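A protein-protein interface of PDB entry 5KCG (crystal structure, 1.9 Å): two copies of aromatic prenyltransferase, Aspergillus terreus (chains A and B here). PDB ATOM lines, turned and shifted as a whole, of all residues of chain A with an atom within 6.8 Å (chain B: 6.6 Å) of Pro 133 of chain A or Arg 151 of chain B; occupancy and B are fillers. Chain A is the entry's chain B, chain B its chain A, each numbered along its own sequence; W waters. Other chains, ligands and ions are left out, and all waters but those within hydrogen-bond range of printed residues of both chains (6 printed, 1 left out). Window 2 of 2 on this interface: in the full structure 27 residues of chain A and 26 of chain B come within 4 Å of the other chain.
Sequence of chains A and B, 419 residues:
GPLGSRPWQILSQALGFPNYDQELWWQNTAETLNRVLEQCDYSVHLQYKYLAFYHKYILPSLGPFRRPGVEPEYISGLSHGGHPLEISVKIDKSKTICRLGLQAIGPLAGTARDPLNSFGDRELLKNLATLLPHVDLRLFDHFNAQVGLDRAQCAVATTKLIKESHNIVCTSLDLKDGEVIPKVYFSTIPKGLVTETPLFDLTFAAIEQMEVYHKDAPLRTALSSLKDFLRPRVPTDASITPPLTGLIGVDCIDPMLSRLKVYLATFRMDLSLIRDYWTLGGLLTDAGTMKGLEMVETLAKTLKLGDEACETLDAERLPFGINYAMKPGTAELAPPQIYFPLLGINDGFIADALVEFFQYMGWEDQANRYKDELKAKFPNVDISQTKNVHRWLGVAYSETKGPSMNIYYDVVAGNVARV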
ATOM      1  N   LEU A 128       1.679 -31.388  19.610  1.00  0.00           N
ATOM      2  CA  LEU A 128       3.043 -31.613  20.148  1.00  0.00           C
ATOM      3  C   LEU A 128       4.065 -30.563  19.847  1.00  0.00           C
ATOM      4  O   LEU A 128       4.968 -30.343  20.688  1.00  0.00           O
ATOM      5  CB  LEU A 128       3.590 -32.990  19.779  1.00  0.00           C
ATOM      6  CG  LEU A 128       2.719 -34.145  20.169  1.00  0.00           C
ATOM      7  CD1 LEU A 128       3.359 -35.500  19.796  1.00  0.00           C
ATOM      8  CD2 LEU A 128       2.334 -34.138  21.595  1.00  0.00           C
ATOM      9  N   ALA A 129       3.968 -29.911  18.648  1.00  0.00           N
ATOM     10  CA  ALA A 129       4.910 -28.896  18.261  1.00  0.00           C
ATOM     11  C   ALA A 129       4.746 -27.680  19.148  1.00  0.00           C
ATOM     12  O   ALA A 129       5.735 -26.970  19.389  1.00  0.00           O
ATOM     13  CB  ALA A 129       4.781 -28.489  16.783  1.00  0.00           C
ATOM     14  N   THR A 130       3.521 -27.351  19.581  1.00  0.00           N
ATOM     15  CA  THR A 130       3.366 -26.258  20.536  1.00  0.00           C
ATOM     16  C   THR A 130       3.731 -26.646  21.975  1.00  0.00           C
ATOM     17  O   THR A 130       4.114 -25.803  22.759  1.00  0.00           O
ATOM     18  CB  THR A 130       1.926 -25.633  20.472  1.00  0.00           C
ATOM     19  OG1 THR A 130       0.975 -26.624  20.765  1.00  0.00           O
ATOM     20  CG2 THR A 130       1.563 -25.141  19.103  1.00  0.00           C
ATOM     21  N   LEU A 131       3.624 -27.933  22.317  1.00  0.00           N
ATOM     22  CA  LEU A 131       4.023 -28.441  23.595  1.00  0.00           C
ATOM     23  C   LEU A 131       5.614 -28.473  23.736  1.00  0.00           C
ATOM     24  O   LEU A 131       6.167 -28.089  24.754  1.00  0.00           O
ATOM     25  CB  LEU A 131       3.431 -29.815  23.806  1.00  0.00           C
ATOM     26  CG  LEU A 131       3.810 -30.513  25.120  1.00  0.00           C
ATOM     27  CD1 LEU A 131       3.222 -29.757  26.298  1.00  0.00           C
ATOM     28  CD2 LEU A 131       3.442 -31.925  25.082  1.00  0.00           C
ATOM     29  N   LEU A 132       6.294 -28.910  22.689  1.00  0.00           N
ATOM     30  CA  LEU A 132       7.693 -29.337  22.749  1.00  0.00           C
ATOM     31  C   LEU A 132       8.542 -28.600  21.743  1.00  0.00           C
ATOM     32  O   LEU A 132       8.326 -28.762  20.542  1.00  0.00           O
ATOM     33  CB  LEU A 132       7.736 -30.803  22.447  1.00  0.00           C
ATOM     34  CG  LEU A 132       6.948 -31.748  23.355  1.00  0.00           C
ATOM     35  CD1 LEU A 132       6.678 -33.079  22.726  1.00  0.00           C
ATOM     36  CD2 LEU A 132       7.633 -31.957  24.705  1.00  0.00           C
ATOM     37  N   PRO A 133       9.551 -27.869  22.197  1.00  0.00           N
ATOM     38  CA  PRO A 133      10.342 -27.019  21.304  1.00  0.00           C
ATOM     39  C   PRO A 133      11.124 -27.779  20.235  1.00  0.00           C
ATOM     40  O   PRO A 133      11.421 -27.234  19.204  1.00  0.00           O
ATOM     41  CB  PRO A 133      11.317 -26.283  22.254  1.00  0.00           C
ATOM     42  CG  PRO A 133      11.254 -27.006  23.562  1.00  0.00           C
ATOM     43  CD  PRO A 133      10.043 -27.870  23.610  1.00  0.00           C
ATOM     44  N   HIS A 134      11.464 -29.033  20.483  1.00  0.00           N
ATOM     45  CA  HIS A 134      12.306 -29.763  19.532  1.00  0.00           C
ATOM     46  C   HIS A 134      11.512 -30.450  18.427  1.00  0.00           C
ATOM     47  O   HIS A 134      12.086 -31.101  17.581  1.00  0.00           O
ATOM     48  CB  HIS A 134      13.121 -30.835  20.295  1.00  0.00           C
ATOM     49  CG  HIS A 134      12.246 -31.794  21.057  1.00  0.00           C
ATOM     50  ND1 HIS A 134      11.653 -31.460  22.274  1.00  0.00           N
ATOM     51  CD2 HIS A 134      11.817 -33.045  20.766  1.00  0.00           C
ATOM     52  CE1 HIS A 134      10.947 -32.489  22.710  1.00  0.00           C
ATOM     53  NE2 HIS A 134      11.039 -33.467  21.824  1.00  0.00           N
ATOM     54  N   VAL A 135      10.189 -30.432  18.478  1.00  0.00           N
ATOM     55  CA  VAL A 135       9.369 -31.142  17.549  1.00  0.00           C
ATOM     56  C   VAL A 135       9.315 -30.259  16.283  1.00  0.00           C
ATOM     57  O   VAL A 135       9.077 -29.077  16.338  1.00  0.00           O
ATOM     58  CB  VAL A 135       7.939 -31.398  18.100  1.00  0.00           C
ATOM     59  CG1 VAL A 135       7.008 -31.919  16.991  1.00  0.00           C
ATOM     60  CG2 VAL A 135       8.042 -32.443  19.155  1.00  0.00           C
ATOM     61  N   ASP A 136       9.532 -30.875  15.156  1.00  0.00           N
ATOM     62  CA  ASP A 136       9.719 -30.161  13.876  1.00  0.00           C
ATOM     63  C   ASP A 136       8.857 -30.987  12.938  1.00  0.00           C
ATOM     64  O   ASP A 136       9.035 -32.213  12.826  1.00  0.00           O
ATOM     65  CB  ASP A 136      11.201 -30.241  13.500  1.00  0.00           C
ATOM     66  CG  ASP A 136      11.564 -29.464  12.250  1.00  0.00           C
ATOM     67  OD1 ASP A 136      10.759 -29.359  11.282  1.00  0.00           O
ATOM     68  OD2 ASP A 136      12.696 -28.985  12.225  1.00  0.00           O
ATOM     69  N   ARG A 138       8.549 -30.547   9.602  1.00  0.00           N
ATOM     70  CA  ARG A 138       8.871 -30.372   8.172  1.00  0.00           C
ATOM     71  C   ARG A 138       9.055 -31.684   7.463  1.00  0.00           C
ATOM     72  O   ARG A 138       8.630 -31.792   6.286  1.00  0.00           O
ATOM     73  CB  ARG A 138      10.060 -29.449   7.994  1.00  0.00           C
ATOM     74  CG  ARG A 138       9.659 -28.023   8.283  1.00  0.00           C
ATOM     75  CD  ARG A 138      10.849 -27.113   8.327  1.00  0.00           C
ATOM     76  NE  ARG A 138      11.831 -27.453   9.354  1.00  0.00           N
ATOM     77  CZ  ARG A 138      12.891 -26.712   9.593  1.00  0.00           C
ATOM     78  NH1 ARG A 138      13.101 -25.648   8.864  1.00  0.00           N
ATOM     79  NH2 ARG A 138      13.726 -27.003  10.559  1.00  0.00           N
ATOM     80  N   GLU A 179      11.956 -36.626  27.994  1.00  0.00           N
ATOM     81  CA  GLU A 179      11.375 -36.010  26.819  1.00  0.00           C
ATOM     82  C   GLU A 179      10.363 -36.919  26.102  1.00  0.00           C
ATOM     83  O   GLU A 179      10.264 -38.138  26.361  1.00  0.00           O
ATOM     84  CB  GLU A 179      12.526 -35.600  25.885  1.00  0.00           C
ATOM     85  CG  GLU A 179      12.980 -34.180  26.142  1.00  0.00           C
ATOM     86  CD  GLU A 179      11.882 -33.153  25.894  1.00  0.00           C
ATOM     87  OE1 GLU A 179      10.769 -33.529  25.428  1.00  0.00           O
ATOM     88  OE2 GLU A 179      12.128 -31.969  26.203  1.00  0.00           O
ATOM     89  N   ALA B 112       6.015 -17.467  22.504  1.00  0.00           N
ATOM     90  CA  ALA B 112       7.183 -18.319  22.322  1.00  0.00           C
ATOM     91  C   ALA B 112       6.856 -19.717  21.732  1.00  0.00           C
ATOM     92  O   ALA B 112       7.678 -20.338  21.002  1.00  0.00           O
ATOM     93  CB  ALA B 112       7.931 -18.463  23.657  1.00  0.00           C
ATOM     94  N   ARG B 113       5.663 -20.219  21.995  1.00  0.00           N
ATOM     95  CA  ARG B 113       5.279 -21.514  21.455  1.00  0.00           C
ATOM     96  C   ARG B 113       4.878 -21.482  19.985  1.00  0.00           C
ATOM     97  O   ARG B 113       4.719 -22.531  19.354  1.00  0.00           O
ATOM     98  CB  ARG B 113       4.171 -22.102  22.297  1.00  0.00           C
ATOM     99  CG  ARG B 113       4.599 -22.481  23.721  1.00  0.00           C
ATOM    100  CD  ARG B 113       3.360 -22.877  24.521  1.00  0.00           C
ATOM    101  NE  ARG B 113       3.720 -23.076  25.925  1.00  0.00           N
ATOM    102  CZ  ARG B 113       4.119 -24.229  26.459  1.00  0.00           C
ATOM    103  NH1 ARG B 113       4.212 -25.332  25.762  1.00  0.00           N
ATOM    104  NH2 ARG B 113       4.442 -24.271  27.743  1.00  0.00           N
ATOM    105  N   ASP B 114       4.657 -20.307  19.443  1.00  0.00           N
ATOM    106  CA  ASP B 114       4.238 -20.197  17.999  1.00  0.00           C
ATOM    107  C   ASP B 114       4.506 -18.783  17.454  1.00  0.00           C
ATOM    108  O   ASP B 114       3.571 -17.968  17.233  1.00  0.00           O
ATOM    109  CB  ASP B 114       2.763 -20.598  17.937  1.00  0.00           C
ATOM    110  CG  ASP B 114       2.177 -20.565  16.520  1.00  0.00           C
ATOM    111  OD1 ASP B 114       2.935 -20.655  15.537  1.00  0.00           O
ATOM    112  OD2 ASP B 114       0.936 -20.413  16.444  1.00  0.00           O
ATOM    113  N   PRO B 115       5.796 -18.383  17.346  1.00  0.00           N
ATOM    114  CA  PRO B 115       6.117 -17.017  17.097  1.00  0.00           C
ATOM    115  C   PRO B 115       5.635 -16.451  15.720  1.00  0.00           C
ATOM    116  O   PRO B 115       5.242 -15.264  15.623  1.00  0.00           O
ATOM    117  CB  PRO B 115       7.649 -16.991  17.202  1.00  0.00           C
ATOM    118  CG  PRO B 115       8.029 -18.239  17.894  1.00  0.00           C
ATOM    119  CD  PRO B 115       6.974 -19.216  17.561  1.00  0.00           C
ATOM    120  N   LEU B 149       9.682 -22.864   9.032  1.00  0.00           N
ATOM    121  CA  LEU B 149      10.793 -22.771   9.965  1.00  0.00           C
ATOM    122  C   LEU B 149      10.484 -23.501  11.269  1.00  0.00           C
ATOM    123  O   LEU B 149       9.342 -23.517  11.714  1.00  0.00           O
ATOM    124  CB  LEU B 149      11.021 -21.320  10.286  1.00  0.00           C
ATOM    125  CG  LEU B 149      11.495 -20.367   9.159  1.00  0.00           C
ATOM    126  CD1 LEU B 149      11.665 -18.960   9.711  1.00  0.00           C
ATOM    127  CD2 LEU B 149      12.808 -20.909   8.623  1.00  0.00           C
ATOM    128  N   ASP B 150      11.499 -24.069  11.910  1.00  0.00           N
ATOM    129  CA  ASP B 150      11.297 -24.623  13.282  1.00  0.00           C
ATOM    130  C   ASP B 150      11.162 -23.536  14.333  1.00  0.00           C
ATOM    131  O   ASP B 150      11.309 -22.342  14.018  1.00  0.00           O
ATOM    132  CB  ASP B 150      12.325 -25.696  13.641  1.00  0.00           C
ATOM    133  CG  ASP B 150      13.701 -25.145  13.897  1.00  0.00           C
ATOM    134  OD1 ASP B 150      13.818 -23.977  14.184  1.00  0.00           O
ATOM    135  OD2 ASP B 150      14.672 -25.919  13.760  1.00  0.00           O
ATOM    136  N   ARG B 151      10.831 -23.900  15.579  1.00  0.00           N
ATOM    137  CA  ARG B 151      10.526 -22.854  16.567  1.00  0.00           C
ATOM    138  C   ARG B 151      11.694 -21.923  16.832  1.00  0.00           C
ATOM    139  O   ARG B 151      11.499 -20.716  16.864  1.00  0.00           O
ATOM    140  CB  ARG B 151      10.045 -23.471  17.896  1.00  0.00           C
ATOM    141  CG  ARG B 151       9.726 -22.432  18.919  1.00  0.00           C
ATOM    142  CD  ARG B 151       9.446 -23.058  20.240  1.00  0.00           C
ATOM    143  NE  ARG B 151       8.296 -23.954  20.246  1.00  0.00           N
ATOM    144  CZ  ARG B 151       7.763 -24.408  21.395  1.00  0.00           C
ATOM    145  NH1 ARG B 151       8.200 -23.970  22.554  1.00  0.00           N
ATOM    146  NH2 ARG B 151       6.771 -25.247  21.412  1.00  0.00           N
ATOM    147  N   ALA B 152      12.910 -22.467  16.988  1.00  0.00           N
ATOM    148  CA  ALA B 152      14.088 -21.595  17.243  1.00  0.00           C
ATOM    149  C   ALA B 152      14.333 -20.649  16.037  1.00  0.00           C
ATOM    150  O   ALA B 152      14.635 -19.477  16.212  1.00  0.00           O
ATOM    151  CB  ALA B 152      15.374 -22.443  17.503  1.00  0.00           C
ATOM    152  N   GLN B 153      14.149 -21.144  14.810  1.00  0.00           N
ATOM    153  CA  GLN B 153      14.267 -20.284  13.636  1.00  0.00           C
ATOM    154  C   GLN B 153      13.158 -19.239  13.601  1.00  0.00           C
ATOM    155  O   GLN B 153      13.406 -18.095  13.175  1.00  0.00           O
ATOM    156  CB  GLN B 153      14.191 -21.115  12.323  1.00  0.00           C
ATOM    157  CG  GLN B 153      15.357 -22.097  12.108  1.00  0.00           C
ATOM    158  CD  GLN B 153      15.153 -22.947  10.839  1.00  0.00           C
ATOM    159  OE1 GLN B 153      14.106 -23.577  10.669  1.00  0.00           O
ATOM    160  NE2 GLN B 153      16.099 -22.856   9.904  1.00  0.00           N
ATOM    161  N   CYS B 154      11.934 -19.602  14.024  1.00  0.00           N
ATOM    162  CA  CYS B 154      10.812 -18.613  14.088  1.00  0.00           C
ATOM    163  C   CYS B 154      11.107 -17.471  15.112  1.00  0.00           C
ATOM    164  O   CYS B 154      10.917 -16.271  14.804  1.00  0.00           O
ATOM    165  CB  CYS B 154       9.489 -19.259  14.458  1.00  0.00           C
ATOM    166  SG  CYS B 154       8.741 -20.301  13.167  1.00  0.00           S
ATOM    167  N   ALA B 155      11.647 -17.864  16.245  1.00  0.00           N
ATOM    168  CA  ALA B 155      12.118 -16.872  17.247  1.00  0.00           C
ATOM    169  C   ALA B 155      13.184 -15.947  16.693  1.00  0.00           C
ATOM    170  O   ALA B 155      13.071 -14.717  16.837  1.00  0.00           O
ATOM    171  CB  ALA B 155      12.632 -17.548  18.488  1.00  0.00           C
ATOM    172  N   VAL B 156      14.197 -16.503  16.033  1.00  0.00           N
ATOM    173  CA  VAL B 156      15.182 -15.639  15.361  1.00  0.00           C
ATOM    174  C   VAL B 156      14.493 -14.705  14.401  1.00  0.00           C
ATOM    175  O   VAL B 156      14.743 -13.486  14.338  1.00  0.00           O
ATOM    176  CB  VAL B 156      16.328 -16.485  14.666  1.00  0.00           C
ATOM    177  CG1 VAL B 156      17.270 -15.588  13.915  1.00  0.00           C
ATOM    178  CG2 VAL B 156      17.133 -17.241  15.680  1.00  0.00           C
HETATM  179  O   HOH W   1      13.434 -25.229  17.699  1.00  0.00           O
HETATM  180  O   HOH W   2      14.272 -28.419  14.056  1.00  0.00           O
HETATM  181  O   HOH W   3       7.325 -25.262  24.820  1.00  0.00           O
HETATM  182  O   HOH W   4      10.920 -26.731  16.481  1.00  0.00           O
HETATM  183  O   HOH W   5       6.533 -23.880  17.971  1.00  0.00           O
HETATM  184  O   HOH W   6      15.495 -24.061   7.181  1.00  0.00           O
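The guanidinium group (NH1) of Arg 113 of chain B lies within hydrogen-bond range of the backbone carbonyl oxygen (O) of Thr 130 of chain A, at 3.0 Å.
The side-chain carboxylate (OD2) of Asp 150 of chain B lies within salt-bridge range of the guanidinium group (NH2) of Arg 138 of chain A, at 3.5 Å.
The guanidinium group (NH2) of Arg 151 of chain B is in hydrogen-bond range of the backbone carbonyl oxygen (O) of Ala 129 of chain A.
The guanidinium group (NH2) of Arg 151 of chain B is in hydrogen-bond range of the backbone carbonyl oxygen (O) of Thr 130 of chain A (3.0 Å).
NH1 of Arg 138 of chain A is in hydrogen-bond range of OE1 of Gln 153 of chain B, 2.9 Å away.
The backbone carbonyl oxygen (O) of Leu 149 of chain B lies within hydrogen-bond range of the side-chain sulfur (SG) of Cys 154 of chain B, at 3.6 Å.
The side-chain carboxylate (OD1) of Asp 150 of chain B sits at hydrogen-bond distance from the backbone NH (N) of Ala 152 of chain B (3.3 Å).
The side-chain carboxylate of Asp 150 of chain B sits at hydrogen-bond distance from the backbone NH of Gln 153 of chain B (2.9 Å).
O of Asp 150 of chain B is in hydrogen-bond range of SG of Cys 154 of chain B.
The guanidinium group (NH2) of Arg 138 of chain A lies within salt-bridge range of the side-chain carboxylate (OD2) of Asp 136 of chain A (2.8 Å).
Among the printed residues, pairs that only touch across the chains: Leu 131 of chain A with Arg 113 of chain B, Asp 136 of chain A with Asp 150 of chain B, Pro 133 of chain A with Arg 151 of chain B, Leu 132 of chain A with Arg 151 of chain B and Arg 138 of chain A with Leu 149 of chain B.
Of the printed residues of chain B, Ala 129 of chain A touches Arg 151 (2.9 Å).
Of chain B, only Arg 151 (3.7 Å) comes within 4 Å of Pro 133 of chain A.
Of the printed residues of chain B, Asp 136 of chain A touches Asp 150.
Of the printed residues of chain B, Arg 138 of chain A touches Leu 149, Asp 150 and Gln 153.
Of the printed residues of chain A, Leu 149 of chain B touches Arg 138 (3.8 Å).
Printed residues of chain A within 4 Å of Arg 151 of chain B: Ala 129, Thr 130, Leu 132 and Pro 133.
Printed residues of chain A within 4 Å of Gln 153 of chain B: Arg 138.
The nearest residue of chain B that does not touch Pro 133 of chain A is Ala 152 of chain B (5.5 Å).
The nearest printed residue of chain B that does not touch Leu 131 of chain A is Arg 151 of chain B (4.1 Å).
Hydrophobic or aromatic side chains of chain A within 4 Å of the printed part of chain B: Pro 133.
Printed residues of chain B that touch a printed residue of chain A: Arg 113, Leu 149, Asp 150, Arg 151 and Gln 153.
Among the printed residues, 10 pairs touch across the chains.
No position is printed for both chains.
Water W2 lies within hydrogen-bond range of OD2 of Asp 136 of chain A (2.5 Å) and OD2 of Asp 150 of chain B (2.5 Å).
Water W5 lies within hydrogen-bond range of O of Arg 113 of chain B (2.7 Å), NE of Arg 151 of chain B (2.9 Å) and O of Ala 129 of chain A (3.5 Å).
Water W3 lies within hydrogen-bond range of the guanidinium group of Arg 151 of chain B, the backbone carbonyl oxygen of Leu 131 of chain A and the guanidinium group of Arg 113 of chain B.
Water W4 lies within hydrogen-bond range of the backbone carbonyl oxygen of Pro 133 of chain A, the backbone NH of Arg 151 of chain B and the backbone carbonyl oxygen of Val 135 of chain A.
Water W1 lies within hydrogen-bond range of N of Ala 152 of chain B (2.9 Å) and O of Pro 133 of chain A (3.2 Å).
Water W6 lies within hydrogen-bond range of the side-chain amide nitrogen of Gln 153 of chain B (3.0 Å) and the guanidinium group of Arg 138 of chain A (3.3 Å).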
